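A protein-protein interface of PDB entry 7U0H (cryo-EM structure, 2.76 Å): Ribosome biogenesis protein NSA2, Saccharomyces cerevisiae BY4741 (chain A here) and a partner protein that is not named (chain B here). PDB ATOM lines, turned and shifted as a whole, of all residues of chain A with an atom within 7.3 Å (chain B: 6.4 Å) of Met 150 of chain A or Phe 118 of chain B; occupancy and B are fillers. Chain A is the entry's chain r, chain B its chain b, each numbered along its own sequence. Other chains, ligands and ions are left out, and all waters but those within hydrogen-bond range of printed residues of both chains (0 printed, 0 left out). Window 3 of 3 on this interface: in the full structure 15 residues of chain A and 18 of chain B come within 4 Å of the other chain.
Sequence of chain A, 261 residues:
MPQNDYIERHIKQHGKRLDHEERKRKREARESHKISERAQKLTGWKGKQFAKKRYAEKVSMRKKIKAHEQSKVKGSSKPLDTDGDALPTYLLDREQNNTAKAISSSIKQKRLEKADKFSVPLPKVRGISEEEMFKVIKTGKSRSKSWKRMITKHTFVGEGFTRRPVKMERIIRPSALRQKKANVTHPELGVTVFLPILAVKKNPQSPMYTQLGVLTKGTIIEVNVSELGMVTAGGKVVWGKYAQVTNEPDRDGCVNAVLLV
Met 150 of chain A touches one residue of chain B.
Of chain A, only Met 150 and Pro 174 come within 4 Å of Phe 118 of chain B.
Printed residues of chain B within 4 Å of Pro 174 of chain A: Phe 118 (3.5 Å).
Of the printed residues of chain A, Arg 114 of chain B touches Ala 176.
Printed residues of chain A within 4 Å of Leu 115 of chain B: Ala 176.
Of the printed residues of chain B, Ala 176 of chain A touches Arg 114 (3.7 Å) and Leu 115 (3.2 Å).
Arg 43 of chain B touches none of the printed residues of chain A.
Arg 149 of chain A touches none of the printed residues of chain B.
The nearest residue of chain B that does not touch Met 150 of chain A is Gln 120 of chain B (5.6 Å).
The nearest residue of chain A that does not touch Phe 118 of chain B is Leu 177 of chain A (4.1 Å).
The side-chain amide oxygen (OE1) of Gln 120 of chain B lies close to the backbone carbonyl oxygen (O) of Phe 118 of chain B (3.3 Å).
Of the 13 printed residues of chain B, 4 touch a printed residue of chain A.
Printed residues of chain A that touch a printed residue of chain B: Met 150, Thr 152, Pro 174 and Ala 176.
Among the printed residues, pairs that only touch across the chains: Ala 176 of chain A with Leu 115 of chain B, Thr 152 of chain A with Gln 120 of chain B, Pro 174 of chain A with Phe 118 of chain B, Met 150 of chain A with Phe 118 of chain B and Ala 176 of chain A with Arg 114 of chain B.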
ATOM      1  N   ARG A 149     -30.351  -9.231  22.445  1.00  0.00           N
ATOM      2  CA  ARG A 149     -29.165  -9.897  22.969  1.00  0.00           C
ATOM      3  C   ARG A 149     -27.901  -9.367  22.312  1.00  0.00           C
ATOM      4  O   ARG A 149     -27.941  -8.833  21.203  1.00  0.00           O
ATOM      5  CB  ARG A 149     -29.256 -11.411  22.756  1.00  0.00           C
ATOM      6  CG  ARG A 149     -29.358 -11.807  21.294  1.00  0.00           C
ATOM      7  CD  ARG A 149     -29.062 -13.281  21.063  1.00  0.00           C
ATOM      8  NE  ARG A 149     -27.644 -13.590  21.206  1.00  0.00           N
ATOM      9  CZ  ARG A 149     -27.135 -14.356  22.160  1.00  0.00           C
ATOM     10  NH1 ARG A 149     -27.903 -14.921  23.079  1.00  0.00           N
ATOM     11  NH2 ARG A 149     -25.822 -14.565  22.191  1.00  0.00           N
ATOM     12  N   MET A 150     -26.775  -9.512  23.005  1.00  0.00           N
ATOM     13  CA  MET A 150     -25.469  -9.222  22.435  1.00  0.00           C
ATOM     14  C   MET A 150     -24.556 -10.422  22.636  1.00  0.00           C
ATOM     15  O   MET A 150     -24.548 -11.035  23.708  1.00  0.00           O
ATOM     16  CB  MET A 150     -24.844  -7.967  23.049  1.00  0.00           C
ATOM     17  CG  MET A 150     -25.158  -7.751  24.514  1.00  0.00           C
ATOM     18  SD  MET A 150     -24.488  -6.189  25.114  1.00  0.00           S
ATOM     19  CE  MET A 150     -22.747  -6.414  24.765  1.00  0.00           C
ATOM     20  N   ILE A 151     -23.801 -10.760  21.594  1.00  0.00           N
ATOM     21  CA  ILE A 151     -22.874 -11.885  21.626  1.00  0.00           C
ATOM     22  C   ILE A 151     -21.507 -11.353  22.039  1.00  0.00           C
ATOM     23  O   ILE A 151     -20.829 -10.682  21.256  1.00  0.00           O
ATOM     24  CB  ILE A 151     -22.813 -12.598  20.269  1.00  0.00           C
ATOM     25  CG1 ILE A 151     -24.215 -13.066  19.866  1.00  0.00           C
ATOM     26  CG2 ILE A 151     -21.810 -13.743  20.303  1.00  0.00           C
ATOM     27  CD1 ILE A 151     -24.287 -14.453  19.283  1.00  0.00           C
ATOM     28  N   THR A 152     -21.088 -11.679  23.264  1.00  0.00           N
ATOM     29  CA  THR A 152     -19.884 -11.118  23.868  1.00  0.00           C
ATOM     30  C   THR A 152     -18.630 -11.932  23.561  1.00  0.00           C
ATOM     31  O   THR A 152     -17.712 -11.986  24.390  1.00  0.00           O
ATOM     32  CB  THR A 152     -20.065 -10.969  25.382  1.00  0.00           C
ATOM     33  OG1 THR A 152     -20.689 -12.144  25.919  1.00  0.00           O
ATOM     34  CG2 THR A 152     -20.910  -9.742  25.708  1.00  0.00           C
ATOM     35  N   LYS A 153     -18.573 -12.584  22.405  1.00  0.00           N
ATOM     36  CA  LYS A 153     -17.376 -13.277  21.958  1.00  0.00           C
ATOM     37  C   LYS A 153     -16.872 -12.638  20.671  1.00  0.00           C
ATOM     38  O   LYS A 153     -17.651 -12.085  19.891  1.00  0.00           O
ATOM     39  CB  LYS A 153     -17.638 -14.771  21.750  1.00  0.00           C
ATOM     40  CG  LYS A 153     -18.019 -15.498  23.022  1.00  0.00           C
ATOM     41  CD  LYS A 153     -17.958 -17.002  22.855  1.00  0.00           C
ATOM     42  CE  LYS A 153     -17.918 -17.688  24.208  1.00  0.00           C
ATOM     43  NZ  LYS A 153     -16.800 -17.174  25.048  1.00  0.00           N
ATOM     44  N   ILE A 171     -29.009  -9.383  15.735  1.00  0.00           N
ATOM     45  CA  ILE A 171     -28.129  -9.644  16.871  1.00  0.00           C
ATOM     46  C   ILE A 171     -27.036  -8.586  16.935  1.00  0.00           C
ATOM     47  O   ILE A 171     -26.191  -8.490  16.039  1.00  0.00           O
ATOM     48  CB  ILE A 171     -27.525 -11.047  16.772  1.00  0.00           C
ATOM     49  CG1 ILE A 171     -28.618 -12.096  16.557  1.00  0.00           C
ATOM     50  CG2 ILE A 171     -26.723 -11.362  18.020  1.00  0.00           C
ATOM     51  CD1 ILE A 171     -29.633 -12.161  17.669  1.00  0.00           C
ATOM     52  N   ILE A 172     -27.031  -7.811  18.016  1.00  0.00           N
ATOM     53  CA  ILE A 172     -26.055  -6.741  18.190  1.00  0.00           C
ATOM     54  C   ILE A 172     -24.710  -7.346  18.565  1.00  0.00           C
ATOM     55  O   ILE A 172     -24.615  -8.148  19.501  1.00  0.00           O
ATOM     56  CB  ILE A 172     -26.530  -5.737  19.255  1.00  0.00           C
ATOM     57  CG1 ILE A 172     -27.789  -5.008  18.782  1.00  0.00           C
ATOM     58  CG2 ILE A 172     -25.438  -4.720  19.562  1.00  0.00           C
ATOM     59  CD1 ILE A 172     -28.255  -3.927  19.737  1.00  0.00           C
ATOM     60  N   ARG A 173     -23.666  -6.964  17.835  1.00  0.00           N
ATOM     61  CA  ARG A 173     -22.310  -7.436  18.091  1.00  0.00           C
ATOM     62  C   ARG A 173     -21.398  -6.237  18.315  1.00  0.00           C
ATOM     63  O   ARG A 173     -21.241  -5.408  17.400  1.00  0.00           O
ATOM     64  CB  ARG A 173     -21.810  -8.294  16.929  1.00  0.00           C
ATOM     65  CG  ARG A 173     -22.705  -9.494  16.640  1.00  0.00           C
ATOM     66  CD  ARG A 173     -22.414 -10.119  15.286  1.00  0.00           C
ATOM     67  NE  ARG A 173     -22.725  -9.223  14.178  1.00  0.00           N
ATOM     68  CZ  ARG A 173     -22.726  -9.586  12.903  1.00  0.00           C
ATOM     69  NH1 ARG A 173     -22.433 -10.823  12.536  1.00  0.00           N
ATOM     70  NH2 ARG A 173     -23.034  -8.686  11.972  1.00  0.00           N
ATOM     71  N   PRO A 174     -20.801  -6.085  19.499  1.00  0.00           N
ATOM     72  CA  PRO A 174     -19.947  -4.915  19.753  1.00  0.00           C
ATOM     73  C   PRO A 174     -18.756  -4.870  18.807  1.00  0.00           C
ATOM     74  O   PRO A 174     -18.175  -5.900  18.456  1.00  0.00           O
ATOM     75  CB  PRO A 174     -19.500  -5.110  21.205  1.00  0.00           C
ATOM     76  CG  PRO A 174     -20.497  -6.051  21.801  1.00  0.00           C
ATOM     77  CD  PRO A 174     -20.926  -6.951  20.684  1.00  0.00           C
ATOM     78  N   SER A 175     -18.389  -3.652  18.403  1.00  0.00           N
ATOM     79  CA  SER A 175     -17.318  -3.480  17.428  1.00  0.00           C
ATOM     80  C   SER A 175     -15.956  -3.825  18.016  1.00  0.00           C
ATOM     81  O   SER A 175     -15.129  -4.457  17.347  1.00  0.00           O
ATOM     82  CB  SER A 175     -17.319  -2.048  16.897  1.00  0.00           C
ATOM     83  OG  SER A 175     -17.203  -1.115  17.955  1.00  0.00           O
ATOM     84  N   ALA A 176     -15.704  -3.426  19.265  1.00  0.00           N
ATOM     85  CA  ALA A 176     -14.380  -3.600  19.851  1.00  0.00           C
ATOM     86  C   ALA A 176     -13.946  -5.058  19.880  1.00  0.00           C
ATOM     87  O   ALA A 176     -12.743  -5.337  19.908  1.00  0.00           O
ATOM     88  CB  ALA A 176     -14.352  -3.012  21.262  1.00  0.00           C
ATOM     89  N   LEU A 177     -14.896  -5.991  19.854  1.00  0.00           N
ATOM     90  CA  LEU A 177     -14.579  -7.409  19.807  1.00  0.00           C
ATOM     91  C   LEU A 177     -14.282  -7.907  18.397  1.00  0.00           C
ATOM     92  O   LEU A 177     -13.887  -9.065  18.240  1.00  0.00           O
ATOM     93  CB  LEU A 177     -15.730  -8.210  20.416  1.00  0.00           C
ATOM     94  CG  LEU A 177     -16.384  -7.578  21.649  1.00  0.00           C
ATOM     95  CD1 LEU A 177     -17.575  -8.397  22.112  1.00  0.00           C
ATOM     96  CD2 LEU A 177     -15.383  -7.406  22.782  1.00  0.00           C
ATOM     97  N   ARG B  43     -14.944  -5.155  36.589  1.00  0.00           N
ATOM     98  CA  ARG B  43     -14.424  -4.489  35.401  1.00  0.00           C
ATOM     99  C   ARG B  43     -13.716  -3.196  35.761  1.00  0.00           C
ATOM    100  O   ARG B  43     -12.667  -2.884  35.194  1.00  0.00           O
ATOM    101  CB  ARG B  43     -15.548  -4.192  34.413  1.00  0.00           C
ATOM    102  CG  ARG B  43     -16.236  -5.395  33.821  1.00  0.00           C
ATOM    103  CD  ARG B  43     -17.035  -4.968  32.606  1.00  0.00           C
ATOM    104  NE  ARG B  43     -18.079  -5.924  32.261  1.00  0.00           N
ATOM    105  CZ  ARG B  43     -19.369  -5.629  32.200  1.00  0.00           C
ATOM    106  NH1 ARG B  43     -19.808  -4.403  32.428  1.00  0.00           N
ATOM    107  NH2 ARG B  43     -20.238  -6.587  31.893  1.00  0.00           N
ATOM    108  N   VAL B 113      -8.482  -1.773  27.648  1.00  0.00           N
ATOM    109  CA  VAL B 113      -9.597  -1.182  28.385  1.00  0.00           C
ATOM    110  C   VAL B 113     -10.882  -1.274  27.568  1.00  0.00           C
ATOM    111  O   VAL B 113     -11.962  -1.576  28.103  1.00  0.00           O
ATOM    112  CB  VAL B 113      -9.267   0.267  28.787  1.00  0.00           C
ATOM    113  CG1 VAL B 113     -10.521   0.999  29.241  1.00  0.00           C
ATOM    114  CG2 VAL B 113      -8.232   0.267  29.894  1.00  0.00           C
ATOM    115  N   ARG B 114     -10.785  -1.045  26.255  1.00  0.00           N
ATOM    116  CA  ARG B 114     -11.952  -1.188  25.389  1.00  0.00           C
ATOM    117  C   ARG B 114     -12.506  -2.609  25.433  1.00  0.00           C
ATOM    118  O   ARG B 114     -13.725  -2.809  25.437  1.00  0.00           O
ATOM    119  CB  ARG B 114     -11.577  -0.795  23.961  1.00  0.00           C
ATOM    120  CG  ARG B 114     -12.721  -0.266  23.128  1.00  0.00           C
ATOM    121  CD  ARG B 114     -12.227   0.270  21.794  1.00  0.00           C
ATOM    122  NE  ARG B 114     -11.450  -0.718  21.053  1.00  0.00           N
ATOM    123  CZ  ARG B 114     -10.169  -0.586  20.737  1.00  0.00           C
ATOM    124  NH1 ARG B 114      -9.486   0.502  21.054  1.00  0.00           N
ATOM    125  NH2 ARG B 114      -9.560  -1.565  20.075  1.00  0.00           N
ATOM    126  N   LEU B 115     -11.623  -3.608  25.461  1.00  0.00           N
ATOM    127  CA  LEU B 115     -12.072  -4.996  25.554  1.00  0.00           C
ATOM    128  C   LEU B 115     -12.652  -5.307  26.933  1.00  0.00           C
ATOM    129  O   LEU B 115     -13.663  -6.010  27.041  1.00  0.00           O
ATOM    130  CB  LEU B 115     -10.921  -5.950  25.233  1.00  0.00           C
ATOM    131  CG  LEU B 115     -10.296  -5.866  23.839  1.00  0.00           C
ATOM    132  CD1 LEU B 115      -9.291  -6.989  23.617  1.00  0.00           C
ATOM    133  CD2 LEU B 115     -11.368  -5.876  22.764  1.00  0.00           C
ATOM    134  N   LEU B 116     -12.019  -4.797  27.995  1.00  0.00           N
ATOM    135  CA  LEU B 116     -12.513  -4.988  29.354  1.00  0.00           C
ATOM    136  C   LEU B 116     -13.882  -4.367  29.563  1.00  0.00           C
ATOM    137  O   LEU B 116     -14.590  -4.767  30.493  1.00  0.00           O
ATOM    138  CB  LEU B 116     -11.529  -4.390  30.362  1.00  0.00           C
ATOM    139  CG  LEU B 116     -10.388  -5.250  30.905  1.00  0.00           C
ATOM    140  CD1 LEU B 116      -9.454  -4.404  31.748  1.00  0.00           C
ATOM    141  CD2 LEU B 116     -10.934  -6.402  31.717  1.00  0.00           C
ATOM    142  N   LYS B 117     -14.255  -3.384  28.737  1.00  0.00           N
ATOM    143  CA  LYS B 117     -15.607  -2.829  28.810  1.00  0.00           C
ATOM    144  C   LYS B 117     -16.672  -3.918  28.856  1.00  0.00           C
ATOM    145  O   LYS B 117     -17.698  -3.756  29.525  1.00  0.00           O
ATOM    146  CB  LYS B 117     -15.878  -1.910  27.615  1.00  0.00           C
ATOM    147  CG  LYS B 117     -15.500  -0.454  27.817  1.00  0.00           C
ATOM    148  CD  LYS B 117     -16.423   0.452  27.010  1.00  0.00           C
ATOM    149  CE  LYS B 117     -16.004   1.913  27.113  1.00  0.00           C
ATOM    150  NZ  LYS B 117     -16.038   2.420  28.516  1.00  0.00           N
ATOM    151  N   PHE B 118     -16.449  -5.036  28.163  1.00  0.00           N
ATOM    152  CA  PHE B 118     -17.432  -6.108  28.061  1.00  0.00           C
ATOM    153  C   PHE B 118     -17.050  -7.337  28.881  1.00  0.00           C
ATOM    154  O   PHE B 118     -17.382  -8.461  28.506  1.00  0.00           O
ATOM    155  CB  PHE B 118     -17.636  -6.493  26.597  1.00  0.00           C
ATOM    156  CG  PHE B 118     -18.159  -5.376  25.751  1.00  0.00           C
ATOM    157  CD1 PHE B 118     -19.518  -5.146  25.653  1.00  0.00           C
ATOM    158  CD2 PHE B 118     -17.291  -4.545  25.061  1.00  0.00           C
ATOM    159  CE1 PHE B 118     -20.004  -4.118  24.878  1.00  0.00           C
ATOM    160  CE2 PHE B 118     -17.772  -3.514  24.290  1.00  0.00           C
ATOM    161  CZ  PHE B 118     -19.130  -3.301  24.196  1.00  0.00           C
ATOM    162  N   GLY B 119     -16.349  -7.142  29.996  1.00  0.00           N
ATOM    163  CA  GLY B 119     -15.984  -8.250  30.856  1.00  0.00           C
ATOM    164  C   GLY B 119     -17.198  -8.983  31.386  1.00  0.00           C
ATOM    165  O   GLY B 119     -18.140  -8.357  31.876  1.00  0.00           O
ATOM    166  N   GLN B 120     -17.196 -10.311  31.281  1.00  0.00           N
ATOM    167  CA  GLN B 120     -18.343 -11.111  31.674  1.00  0.00           C
ATOM    168  C   GLN B 120     -18.126 -11.908  32.951  1.00  0.00           C
ATOM    169  O   GLN B 120     -19.091 -12.470  33.477  1.00  0.00           O
ATOM    170  CB  GLN B 120     -18.735 -12.067  30.537  1.00  0.00           C
ATOM    171  CG  GLN B 120     -19.197 -11.359  29.274  1.00  0.00           C
ATOM    172  CD  GLN B 120     -20.404 -10.473  29.510  1.00  0.00           C
ATOM    173  OE1 GLN B 120     -20.474  -9.349  29.006  1.00  0.00           O
ATOM    174  NE2 GLN B 120     -21.364 -10.974  30.278  1.00  0.00           N
ATOM    175  N   SER B 121     -16.900 -11.974  33.463  1.00  0.00           N
ATOM    176  CA  SER B 121     -16.636 -12.650  34.724  1.00  0.00           C
ATOM    177  C   SER B 121     -15.318 -12.146  35.285  1.00  0.00           C
ATOM    178  O   SER B 121     -14.508 -11.541  34.575  1.00  0.00           O
ATOM    179  CB  SER B 121     -16.592 -14.172  34.555  1.00  0.00           C
ATOM    180  OG  SER B 121     -15.345 -14.581  34.021  1.00  0.00           O
ATOM    181  N   GLN B 124     -12.447 -13.884  33.346  1.00  0.00           N
ATOM    182  CA  GLN B 124     -12.117 -13.304  32.049  1.00  0.00           C
ATOM    183  C   GLN B 124     -11.485 -11.926  32.203  1.00  0.00           C
ATOM    184  O   GLN B 124     -10.550 -11.582  31.468  1.00  0.00           O
ATOM    185  CB  GLN B 124     -13.366 -13.240  31.169  1.00  0.00           C
ATOM    186  CG  GLN B 124     -13.074 -12.933  29.713  1.00  0.00           C
ATOM    187  CD  GLN B 124     -14.299 -13.054  28.830  1.00  0.00           C
ATOM    188  OE1 GLN B 124     -15.022 -14.052  28.881  1.00  0.00           O
ATOM    189  NE2 GLN B 124     -14.543 -12.036  28.015  1.00  0.00           N
ATOM    190  N   CYS B 125     -11.977 -11.125  33.152  1.00  0.00           N
ATOM    191  CA  CYS B 125     -11.375  -9.817  33.394  1.00  0.00           C
ATOM    192  C   CYS B 125      -9.928  -9.950  33.850  1.00  0.00           C
ATOM    193  O   CYS B 125      -9.053  -9.206  33.391  1.00  0.00           O
ATOM    194  CB  CYS B 125     -12.199  -9.044  34.423  1.00  0.00           C
ATOM    195  SG  CYS B 125     -13.819  -8.506  33.837  1.00  0.00           S
ATOM    196  N   LEU B 128      -7.786 -10.837  30.819  1.00  0.00           N
ATOM    197  CA  LEU B 128      -7.497  -9.675  29.983  1.00  0.00           C
ATOM    198  C   LEU B 128      -6.463  -8.764  30.638  1.00  0.00           C
ATOM    199  O   LEU B 128      -5.576  -8.228  29.961  1.00  0.00           O
ATOM    200  CB  LEU B 128      -8.786  -8.907  29.688  1.00  0.00           C
ATOM    201  CG  LEU B 128      -9.820  -9.570  28.775  1.00  0.00           C
ATOM    202  CD1 LEU B 128     -11.095  -8.752  28.740  1.00  0.00           C
ATOM    203  CD2 LEU B 128      -9.274  -9.739  27.373  1.00  0.00           C
